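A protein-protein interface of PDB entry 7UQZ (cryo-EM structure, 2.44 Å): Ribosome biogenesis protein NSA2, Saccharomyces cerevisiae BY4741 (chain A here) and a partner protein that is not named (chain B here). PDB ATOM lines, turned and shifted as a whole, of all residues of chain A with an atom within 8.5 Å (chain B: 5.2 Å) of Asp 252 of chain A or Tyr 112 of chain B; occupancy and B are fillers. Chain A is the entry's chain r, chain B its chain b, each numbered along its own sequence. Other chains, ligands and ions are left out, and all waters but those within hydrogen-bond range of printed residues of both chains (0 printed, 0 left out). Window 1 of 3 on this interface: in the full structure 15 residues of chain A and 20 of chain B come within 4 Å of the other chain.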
ATOM      1  N   HIS A 154     -20.987  19.125  17.507  1.00  0.00           N
ATOM      2  CA  HIS A 154     -20.628  20.535  17.521  1.00  0.00           C
ATOM      3  C   HIS A 154     -20.818  21.149  16.140  1.00  0.00           C
ATOM      4  O   HIS A 154     -20.547  20.512  15.119  1.00  0.00           O
ATOM      5  CB  HIS A 154     -19.184  20.717  17.988  1.00  0.00           C
ATOM      6  CG  HIS A 154     -18.988  20.458  19.449  1.00  0.00           C
ATOM      7  ND1 HIS A 154     -18.563  21.432  20.327  1.00  0.00           N
ATOM      8  CD2 HIS A 154     -19.169  19.340  20.189  1.00  0.00           C
ATOM      9  CE1 HIS A 154     -18.486  20.922  21.544  1.00  0.00           C
ATOM     10  NE2 HIS A 154     -18.847  19.653  21.486  1.00  0.00           N
ATOM     11  N   GLN A 179     -19.339  26.404  18.032  1.00  0.00           N
ATOM     12  CA  GLN A 179     -17.922  26.718  18.111  1.00  0.00           C
ATOM     13  C   GLN A 179     -17.594  27.901  17.211  1.00  0.00           C
ATOM     14  O   GLN A 179     -18.206  28.091  16.157  1.00  0.00           O
ATOM     15  CB  GLN A 179     -17.060  25.512  17.707  1.00  0.00           C
ATOM     16  CG  GLN A 179     -17.153  24.322  18.648  1.00  0.00           C
ATOM     17  CD  GLN A 179     -16.260  24.464  19.866  1.00  0.00           C
ATOM     18  OE1 GLN A 179     -15.587  25.478  20.044  1.00  0.00           O
ATOM     19  NE2 GLN A 179     -16.247  23.440  20.708  1.00  0.00           N
ATOM     20  N   ASN A 183      -8.053  24.981  17.378  1.00  0.00           N
ATOM     21  CA  ASN A 183      -6.604  24.867  17.498  1.00  0.00           C
ATOM     22  C   ASN A 183      -6.072  24.288  16.192  1.00  0.00           C
ATOM     23  O   ASN A 183      -6.248  23.098  15.916  1.00  0.00           O
ATOM     24  CB  ASN A 183      -6.219  23.988  18.685  1.00  0.00           C
ATOM     25  CG  ASN A 183      -6.875  24.430  19.978  1.00  0.00           C
ATOM     26  OD1 ASN A 183      -6.504  25.448  20.557  1.00  0.00           O
ATOM     27  ND2 ASN A 183      -7.846  23.656  20.443  1.00  0.00           N
ATOM     28  N   LYS A 217     -15.038  14.787  12.788  1.00  0.00           N
ATOM     29  CA  LYS A 217     -13.706  14.430  12.323  1.00  0.00           C
ATOM     30  C   LYS A 217     -13.679  14.320  10.803  1.00  0.00           C
ATOM     31  O   LYS A 217     -14.602  13.782  10.186  1.00  0.00           O
ATOM     32  CB  LYS A 217     -13.261  13.114  12.957  1.00  0.00           C
ATOM     33  CG  LYS A 217     -11.772  12.841  12.859  1.00  0.00           C
ATOM     34  CD  LYS A 217     -11.396  11.588  13.625  1.00  0.00           C
ATOM     35  CE  LYS A 217      -9.920  11.282  13.491  1.00  0.00           C
ATOM     36  NZ  LYS A 217      -9.545  10.032  14.206  1.00  0.00           N
ATOM     37  N   VAL A 245     -10.326  18.928  10.238  1.00  0.00           N
ATOM     38  CA  VAL A 245     -10.513  18.572  11.640  1.00  0.00           C
ATOM     39  C   VAL A 245      -9.991  17.161  11.874  1.00  0.00           C
ATOM     40  O   VAL A 245     -10.312  16.229  11.125  1.00  0.00           O
ATOM     41  CB  VAL A 245     -11.994  18.700  12.031  1.00  0.00           C
ATOM     42  CG1 VAL A 245     -12.211  18.296  13.480  1.00  0.00           C
ATOM     43  CG2 VAL A 245     -12.483  20.120  11.800  1.00  0.00           C
ATOM     44  N   THR A 246      -9.176  16.998  12.916  1.00  0.00           N
ATOM     45  CA  THR A 246      -8.493  15.741  13.186  1.00  0.00           C
ATOM     46  C   THR A 246      -8.975  15.041  14.450  1.00  0.00           C
ATOM     47  O   THR A 246      -8.452  13.973  14.781  1.00  0.00           O
ATOM     48  CB  THR A 246      -6.980  15.972  13.291  1.00  0.00           C
ATOM     49  OG1 THR A 246      -6.712  16.980  14.273  1.00  0.00           O
ATOM     50  CG2 THR A 246      -6.411  16.408  11.957  1.00  0.00           C
ATOM     51  N   ASN A 247      -9.949  15.598  15.162  1.00  0.00           N
ATOM     52  CA  ASN A 247     -10.401  15.031  16.423  1.00  0.00           C
ATOM     53  C   ASN A 247     -11.919  14.923  16.423  1.00  0.00           C
ATOM     54  O   ASN A 247     -12.588  15.225  15.431  1.00  0.00           O
ATOM     55  CB  ASN A 247      -9.921  15.870  17.613  1.00  0.00           C
ATOM     56  CG  ASN A 247     -10.637  17.203  17.717  1.00  0.00           C
ATOM     57  OD1 ASN A 247     -10.931  17.847  16.712  1.00  0.00           O
ATOM     58  ND2 ASN A 247     -10.918  17.625  18.942  1.00  0.00           N
ATOM     59  N   GLU A 248     -12.463  14.491  17.559  1.00  0.00           N
ATOM     60  CA  GLU A 248     -13.904  14.463  17.773  1.00  0.00           C
ATOM     61  C   GLU A 248     -14.259  15.502  18.827  1.00  0.00           C
ATOM     62  O   GLU A 248     -14.118  15.242  20.036  1.00  0.00           O
ATOM     63  CB  GLU A 248     -14.370  13.068  18.205  1.00  0.00           C
ATOM     64  CG  GLU A 248     -14.111  11.966  17.178  1.00  0.00           C
ATOM     65  CD  GLU A 248     -15.136  11.931  16.049  1.00  0.00           C
ATOM     66  OE1 GLU A 248     -15.945  12.873  15.924  1.00  0.00           O
ATOM     67  OE2 GLU A 248     -15.134  10.946  15.281  1.00  0.00           O
ATOM     68  N   PRO A 249     -14.689  16.699  18.421  1.00  0.00           N
ATOM     69  CA  PRO A 249     -15.031  17.736  19.406  1.00  0.00           C
ATOM     70  C   PRO A 249     -16.168  17.350  20.330  1.00  0.00           C
ATOM     71  O   PRO A 249     -16.179  17.791  21.482  1.00  0.00           O
ATOM     72  CB  PRO A 249     -15.386  18.951  18.534  1.00  0.00           C
ATOM     73  CG  PRO A 249     -15.586  18.419  17.164  1.00  0.00           C
ATOM     74  CD  PRO A 249     -14.738  17.205  17.040  1.00  0.00           C
ATOM     75  N   ASP A 250     -17.118  16.531  19.876  1.00  0.00           N
ATOM     76  CA  ASP A 250     -18.151  16.044  20.782  1.00  0.00           C
ATOM     77  C   ASP A 250     -17.587  15.129  21.862  1.00  0.00           C
ATOM     78  O   ASP A 250     -18.225  14.957  22.905  1.00  0.00           O
ATOM     79  CB  ASP A 250     -19.246  15.320  20.000  1.00  0.00           C
ATOM     80  CG  ASP A 250     -18.693  14.283  19.048  1.00  0.00           C
ATOM     81  OD1 ASP A 250     -17.843  14.642  18.206  1.00  0.00           O
ATOM     82  OD2 ASP A 250     -19.103  13.109  19.144  1.00  0.00           O
ATOM     83  N   ARG A 251     -16.407  14.551  21.642  1.00  0.00           N
ATOM     84  CA  ARG A 251     -15.762  13.714  22.644  1.00  0.00           C
ATOM     85  C   ARG A 251     -14.826  14.500  23.554  1.00  0.00           C
ATOM     86  O   ARG A 251     -14.800  14.249  24.762  1.00  0.00           O
ATOM     87  CB  ARG A 251     -14.979  12.581  21.975  1.00  0.00           C
ATOM     88  CG  ARG A 251     -15.827  11.490  21.350  1.00  0.00           C
ATOM     89  CD  ARG A 251     -14.938  10.392  20.794  1.00  0.00           C
ATOM     90  NE  ARG A 251     -15.630   9.543  19.832  1.00  0.00           N
ATOM     91  CZ  ARG A 251     -15.038   8.605  19.106  1.00  0.00           C
ATOM     92  NH1 ARG A 251     -13.741   8.364  19.210  1.00  0.00           N
ATOM     93  NH2 ARG A 251     -15.765   7.888  18.253  1.00  0.00           N
ATOM     94  N   ASP A 252     -14.043  15.436  23.014  1.00  0.00           N
ATOM     95  CA  ASP A 252     -13.005  16.076  23.819  1.00  0.00           C
ATOM     96  C   ASP A 252     -13.253  17.558  24.096  1.00  0.00           C
ATOM     97  O   ASP A 252     -12.396  18.209  24.704  1.00  0.00           O
ATOM     98  CB  ASP A 252     -11.631  15.876  23.171  1.00  0.00           C
ATOM     99  CG  ASP A 252     -11.625  16.174  21.692  1.00  0.00           C
ATOM    100  OD1 ASP A 252     -12.353  17.086  21.253  1.00  0.00           O
ATOM    101  OD2 ASP A 252     -10.887  15.481  20.959  1.00  0.00           O
ATOM    102  N   GLY A 253     -14.395  18.106  23.690  1.00  0.00           N
ATOM    103  CA  GLY A 253     -14.750  19.465  24.051  1.00  0.00           C
ATOM    104  C   GLY A 253     -14.038  20.569  23.301  1.00  0.00           C
ATOM    105  O   GLY A 253     -14.210  21.739  23.652  1.00  0.00           O
ATOM    106  N   CYS A 254     -13.249  20.246  22.279  1.00  0.00           N
ATOM    107  CA  CYS A 254     -12.511  21.264  21.544  1.00  0.00           C
ATOM    108  C   CYS A 254     -12.313  20.804  20.110  1.00  0.00           C
ATOM    109  O   CYS A 254     -12.401  19.613  19.801  1.00  0.00           O
ATOM    110  CB  CYS A 254     -11.155  21.562  22.195  1.00  0.00           C
ATOM    111  SG  CYS A 254      -9.994  20.175  22.173  1.00  0.00           S
ATOM    112  N   VAL A 255     -12.023  21.762  19.237  1.00  0.00           N
ATOM    113  CA  VAL A 255     -11.819  21.496  17.818  1.00  0.00           C
ATOM    114  C   VAL A 255     -10.330  21.594  17.520  1.00  0.00           C
ATOM    115  O   VAL A 255      -9.709  22.638  17.747  1.00  0.00           O
ATOM    116  CB  VAL A 255     -12.623  22.469  16.942  1.00  0.00           C
ATOM    117  CG1 VAL A 255     -12.436  22.135  15.474  1.00  0.00           C
ATOM    118  CG2 VAL A 255     -14.094  22.433  17.319  1.00  0.00           C
ATOM    119  N   ASN A 256      -9.759  20.504  17.018  1.00  0.00           N
ATOM    120  CA  ASN A 256      -8.375  20.454  16.575  1.00  0.00           C
ATOM    121  C   ASN A 256      -8.342  20.233  15.071  1.00  0.00           C
ATOM    122  O   ASN A 256      -9.058  19.376  14.546  1.00  0.00           O
ATOM    123  CB  ASN A 256      -7.606  19.335  17.283  1.00  0.00           C
ATOM    124  CG  ASN A 256      -7.517  19.543  18.781  1.00  0.00           C
ATOM    125  OD1 ASN A 256      -7.390  20.669  19.255  1.00  0.00           O
ATOM    126  ND2 ASN A 256      -7.579  18.452  19.535  1.00  0.00           N
ATOM    127  N   VAL B  50     -16.640  16.180  37.799  1.00  0.00           N
ATOM    128  CA  VAL B  50     -15.978  17.393  37.311  1.00  0.00           C
ATOM    129  C   VAL B  50     -16.115  18.527  38.324  1.00  0.00           C
ATOM    130  O   VAL B  50     -15.139  19.221  38.648  1.00  0.00           O
ATOM    131  CB  VAL B  50     -16.538  17.794  35.933  1.00  0.00           C
ATOM    132  CG1 VAL B  50     -15.993  19.146  35.500  1.00  0.00           C
ATOM    133  CG2 VAL B  50     -16.199  16.738  34.897  1.00  0.00           C
ATOM    134  N   GLN B 107     -13.330  28.150  34.906  1.00  0.00           N
ATOM    135  CA  GLN B 107     -13.872  28.200  33.549  1.00  0.00           C
ATOM    136  C   GLN B 107     -13.966  26.809  32.931  1.00  0.00           C
ATOM    137  O   GLN B 107     -14.971  26.476  32.286  1.00  0.00           O
ATOM    138  CB  GLN B 107     -13.021  29.120  32.677  1.00  0.00           C
ATOM    139  CG  GLN B 107     -13.623  29.388  31.311  1.00  0.00           C
ATOM    140  CD  GLN B 107     -14.988  30.043  31.398  1.00  0.00           C
ATOM    141  OE1 GLN B 107     -15.119  31.168  31.876  1.00  0.00           O
ATOM    142  NE2 GLN B 107     -16.014  29.336  30.942  1.00  0.00           N
ATOM    143  N   VAL B 108     -12.933  25.980  33.119  1.00  0.00           N
ATOM    144  CA  VAL B 108     -12.961  24.618  32.585  1.00  0.00           C
ATOM    145  C   VAL B 108     -14.102  23.823  33.207  1.00  0.00           C
ATOM    146  O   VAL B 108     -14.834  23.106  32.507  1.00  0.00           O
ATOM    147  CB  VAL B 108     -11.601  23.927  32.803  1.00  0.00           C
ATOM    148  CG1 VAL B 108     -11.708  22.434  32.530  1.00  0.00           C
ATOM    149  CG2 VAL B 108     -10.544  24.541  31.906  1.00  0.00           C
ATOM    150  N   ALA B 109     -14.286  23.953  34.525  1.00  0.00           N
ATOM    151  CA  ALA B 109     -15.360  23.232  35.203  1.00  0.00           C
ATOM    152  C   ALA B 109     -16.730  23.634  34.664  1.00  0.00           C
ATOM    153  O   ALA B 109     -17.566  22.772  34.361  1.00  0.00           O
ATOM    154  CB  ALA B 109     -15.279  23.476  36.711  1.00  0.00           C
ATOM    155  N   ARG B 110     -16.971  24.942  34.521  1.00  0.00           N
ATOM    156  CA  ARG B 110     -18.263  25.403  34.014  1.00  0.00           C
ATOM    157  C   ARG B 110     -18.509  24.915  32.589  1.00  0.00           C
ATOM    158  O   ARG B 110     -19.589  24.390  32.274  1.00  0.00           O
ATOM    159  CB  ARG B 110     -18.346  26.929  34.075  1.00  0.00           C
ATOM    160  CG  ARG B 110     -18.691  27.491  35.441  1.00  0.00           C
ATOM    161  CD  ARG B 110     -18.965  28.985  35.362  1.00  0.00           C
ATOM    162  NE  ARG B 110     -17.837  29.713  34.796  1.00  0.00           N
ATOM    163  CZ  ARG B 110     -16.910  30.334  35.512  1.00  0.00           C
ATOM    164  NH1 ARG B 110     -16.960  30.360  36.834  1.00  0.00           N
ATOM    165  NH2 ARG B 110     -15.909  30.945  34.887  1.00  0.00           N
ATOM    166  N   ASP B 111     -17.503  25.066  31.718  1.00  0.00           N
ATOM    167  CA  ASP B 111     -17.660  24.676  30.321  1.00  0.00           C
ATOM    168  C   ASP B 111     -17.935  23.186  30.184  1.00  0.00           C
ATOM    169  O   ASP B 111     -18.788  22.773  29.389  1.00  0.00           O
ATOM    170  CB  ASP B 111     -16.411  25.054  29.524  1.00  0.00           C
ATOM    171  CG  ASP B 111     -16.214  26.550  29.421  1.00  0.00           C
ATOM    172  OD1 ASP B 111     -17.062  27.302  29.942  1.00  0.00           O
ATOM    173  OD2 ASP B 111     -15.203  26.973  28.823  1.00  0.00           O
ATOM    174  N   TYR B 112     -17.236  22.358  30.961  1.00  0.00           N
ATOM    175  CA  TYR B 112     -17.414  20.926  30.780  1.00  0.00           C
ATOM    176  C   TYR B 112     -18.663  20.394  31.467  1.00  0.00           C
ATOM    177  O   TYR B 112     -19.218  19.394  31.009  1.00  0.00           O
ATOM    178  CB  TYR B 112     -16.168  20.179  31.234  1.00  0.00           C
ATOM    179  CG  TYR B 112     -15.159  20.091  30.118  1.00  0.00           C
ATOM    180  CD1 TYR B 112     -15.176  19.028  29.226  1.00  0.00           C
ATOM    181  CD2 TYR B 112     -14.217  21.091  29.929  1.00  0.00           C
ATOM    182  CE1 TYR B 112     -14.268  18.952  28.193  1.00  0.00           C
ATOM    183  CE2 TYR B 112     -13.304  21.023  28.901  1.00  0.00           C
ATOM    184  CZ  TYR B 112     -13.335  19.952  28.035  1.00  0.00           C
ATOM    185  OH  TYR B 112     -12.426  19.882  27.008  1.00  0.00           O
ATOM    186  N   VAL B 113     -19.159  21.052  32.519  1.00  0.00           N
ATOM    187  CA  VAL B 113     -20.491  20.701  33.011  1.00  0.00           C
ATOM    188  C   VAL B 113     -21.546  21.021  31.956  1.00  0.00           C
ATOM    189  O   VAL B 113     -22.454  20.214  31.685  1.00  0.00           O
ATOM    190  CB  VAL B 113     -20.779  21.413  34.346  1.00  0.00           C
ATOM    191  CG1 VAL B 113     -22.246  21.283  34.714  1.00  0.00           C
ATOM    192  CG2 VAL B 113     -19.915  20.829  35.449  1.00  0.00           C
ATOM    193  N   ARG B 114     -21.422  22.191  31.316  1.00  0.00           N
ATOM    194  CA  ARG B 114     -22.370  22.557  30.267  1.00  0.00           C
ATOM    195  C   ARG B 114     -22.320  21.576  29.101  1.00  0.00           C
ATOM    196  O   ARG B 114     -23.360  21.223  28.534  1.00  0.00           O
ATOM    197  CB  ARG B 114     -22.094  23.980  29.785  1.00  0.00           C
ATOM    198  CG  ARG B 114     -23.267  24.631  29.077  1.00  0.00           C
ATOM    199  CD  ARG B 114     -22.917  26.017  28.556  1.00  0.00           C
ATOM    200  NE  ARG B 114     -22.375  26.877  29.600  1.00  0.00           N
ATOM    201  CZ  ARG B 114     -21.106  27.257  29.677  1.00  0.00           C
ATOM    202  NH1 ARG B 114     -20.218  26.886  28.770  1.00  0.00           N
ATOM    203  NH2 ARG B 114     -20.720  28.024  30.691  1.00  0.00           N
ATOM    204  N   LEU B 115     -21.120  21.121  28.727  1.00  0.00           N
ATOM    205  CA  LEU B 115     -21.009  20.126  27.662  1.00  0.00           C
ATOM    206  C   LEU B 115     -21.557  18.771  28.095  1.00  0.00           C
ATOM    207  O   LEU B 115     -22.204  18.078  27.301  1.00  0.00           O
ATOM    208  CB  LEU B 115     -19.558  19.992  27.205  1.00  0.00           C
ATOM    209  CG  LEU B 115     -18.999  21.145  26.372  1.00  0.00           C
ATOM    210  CD1 LEU B 115     -17.561  20.864  25.999  1.00  0.00           C
ATOM    211  CD2 LEU B 115     -19.844  21.375  25.131  1.00  0.00           C
ATOM    212  N   LEU B 116     -21.312  18.373  29.349  1.00  0.00           N
ATOM    213  CA  LEU B 116     -21.839  17.111  29.857  1.00  0.00           C
ATOM    214  C   LEU B 116     -23.355  17.101  29.917  1.00  0.00           C
ATOM    215  O   LEU B 116     -23.950  16.022  29.988  1.00  0.00           O
ATOM    216  CB  LEU B 116     -21.275  16.821  31.248  1.00  0.00           C
ATOM    217  CG  LEU B 116     -19.939  16.088  31.329  1.00  0.00           C
ATOM    218  CD1 LEU B 116     -19.452  16.055  32.763  1.00  0.00           C
ATOM    219  CD2 LEU B 116     -20.071  14.680  30.772  1.00  0.00           C
ATOM    220  N   LYS B 117     -23.992  18.274  29.913  1.00  0.00           N
ATOM    221  CA  LYS B 117     -25.449  18.311  29.797  1.00  0.00           C
ATOM    222  C   LYS B 117     -25.965  17.651  28.518  1.00  0.00           C
ATOM    223  O   LYS B 117     -27.126  17.231  28.481  1.00  0.00           O
ATOM    224  CB  LYS B 117     -25.959  19.750  29.852  1.00  0.00           C
ATOM    225  CG  LYS B 117     -25.994  20.357  31.239  1.00  0.00           C
ATOM    226  CD  LYS B 117     -26.230  21.855  31.162  1.00  0.00           C
ATOM    227  CE  LYS B 117     -27.456  22.182  30.330  1.00  0.00           C
ATOM    228  NZ  LYS B 117     -27.631  23.650  30.161  1.00  0.00           N
ATOM    229  N   LEU B 128     -15.617  13.206  28.166  1.00  0.00           N
ATOM    230  CA  LEU B 128     -15.722  14.618  28.534  1.00  0.00           C
ATOM    231  C   LEU B 128     -15.195  14.870  29.944  1.00  0.00           C
ATOM    232  O   LEU B 128     -14.497  15.866  30.186  1.00  0.00           O
ATOM    233  CB  LEU B 128     -17.171  15.090  28.404  1.00  0.00           C
ATOM    234  CG  LEU B 128     -17.713  15.256  26.982  1.00  0.00           C
ATOM    235  CD1 LEU B 128     -19.182  15.644  27.006  1.00  0.00           C
ATOM    236  CD2 LEU B 128     -16.906  16.288  26.212  1.00  0.00           C
ATOM    237  N   ALA B 131     -11.456  14.644  29.849  1.00  0.00           N
ATOM    238  CA  ALA B 131     -10.925  15.856  29.235  1.00  0.00           C
ATOM    239  C   ALA B 131     -10.888  17.013  30.224  1.00  0.00           C
ATOM    240  O   ALA B 131      -9.895  17.748  30.294  1.00  0.00           O
ATOM    241  CB  ALA B 131     -11.753  16.227  28.007  1.00  0.00           C
ATOM    242  N   ALA B 132     -11.966  17.189  30.994  1.00  0.00           N
ATOM    243  CA  ALA B 132     -12.001  18.258  31.989  1.00  0.00           C
ATOM    244  C   ALA B 132     -10.906  18.072  33.034  1.00  0.00           C
ATOM    245  O   ALA B 132     -10.174  19.018  33.365  1.00  0.00           O
ATOM    246  CB  ALA B 132     -13.376  18.309  32.653  1.00  0.00           C
ATOM    247  N   ARG B 135      -7.392  18.748  31.495  1.00  0.00           N
ATOM    248  CA  ARG B 135      -7.120  20.174  31.338  1.00  0.00           C
ATOM    249  C   ARG B 135      -6.817  20.832  32.680  1.00  0.00           C
ATOM    250  O   ARG B 135      -5.900  21.662  32.780  1.00  0.00           O
ATOM    251  CB  ARG B 135      -8.295  20.858  30.639  1.00  0.00           C
ATOM    252  CG  ARG B 135      -8.434  20.473  29.172  1.00  0.00           C
ATOM    253  CD  ARG B 135      -9.738  20.972  28.577  1.00  0.00           C
ATOM    254  NE  ARG B 135      -9.741  22.415  28.368  1.00  0.00           N
ATOM    255  CZ  ARG B 135      -9.815  23.000  27.181  1.00  0.00           C
ATOM    256  NH1 ARG B 135      -9.922  22.294  26.067  1.00  0.00           N
ATOM    257  NH2 ARG B 135      -9.791  24.327  27.108  1.00  0.00           N
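The side-chain hydroxyl (OH) of Tyr 112 of chain B lies within hydrogen-bond range of the backbone carbonyl oxygen (O) of Asp 252 of chain A, 2.8 Å away.
The backbone carbonyl oxygen (O) of Pro 249 of chain A sits at hydrogen-bond distance from a ring nitrogen (NE2) of His 154 of chain A (3.3 Å). The side-chain carboxylate (OD1) of Asp 252 of chain A lies close to the backbone NH (N) of Cys 254 of chain A, 3.4 Å away. The side-chain carboxylate of Asp 252 of chain A is in hydrogen-bond range of the side-chain amide nitrogen of Asn 247 of chain A (2.8 Å). A ring nitrogen (ND1) of His 154 of chain A sits at hydrogen-bond distance from the side-chain amide nitrogen (NE2) of Gln 179 of chain A (3.1 Å).
Of the 16 printed residues of chain B, 4 touch a printed residue of chain A. Printed residues of chain B that touch a printed residue of chain A: Tyr 112, Leu 115, Leu 128 and Ala 131. Along chain B the printed residues that touch a printed residue of chain A span positions 112 to 131. Among the printed residues, 8 pairs touch across the chains. Among the printed residues, no Asp or Glu carboxylate lies within 4 Å of a Lys or Arg side-chain nitrogen of the other chain.
Of the printed residues of chain B, Arg 251 of chain A touches Leu 128 (3.3 Å). Asp 252 of chain A touches just these residues of chain B: Tyr 112 and Ala 131. Printed residues of chain B within 4 Å of Gly 253 of chain A: Tyr 112, Leu 115 and Leu 128. Ala 109 of chain B touches none of the printed residues of chain A. Of chain A, only Asp 252 (2.8 Å) and Gly 253 (3.8 Å) come within 4 Å of Tyr 112 of chain B. Printed residues of chain A within 4 Å of Leu 115 of chain B: His 154 and Gly 253. Printed residues of chain A within 4 Å of Leu 128 of chain B: Asp 250 (3.8 Å), Arg 251 (3.3 Å) and Gly 253 (3.996 Å). The nearest residue of chain A that does not touch Tyr 112 of chain B is Cys 254 of chain A (4.8 Å).
Among the printed residues, merely in contact across the chains: Arg 251 of chain A with Leu 128 of chain B (3.3 Å), Gly 253 of chain A with Leu 115 of chain B (3.7 Å), Gly 253 of chain A with Tyr 112 of chain B (3.8 Å), Asp 250 of chain A with Leu 128 of chain B (3.8 Å), His 154 of chain A with Leu 115 of chain B (3.9 Å), Asp 252 of chain A with Ala 131 of chain B (3.9 Å) and Gly 253 of chain A with Leu 128 of chain B (3.996 Å).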
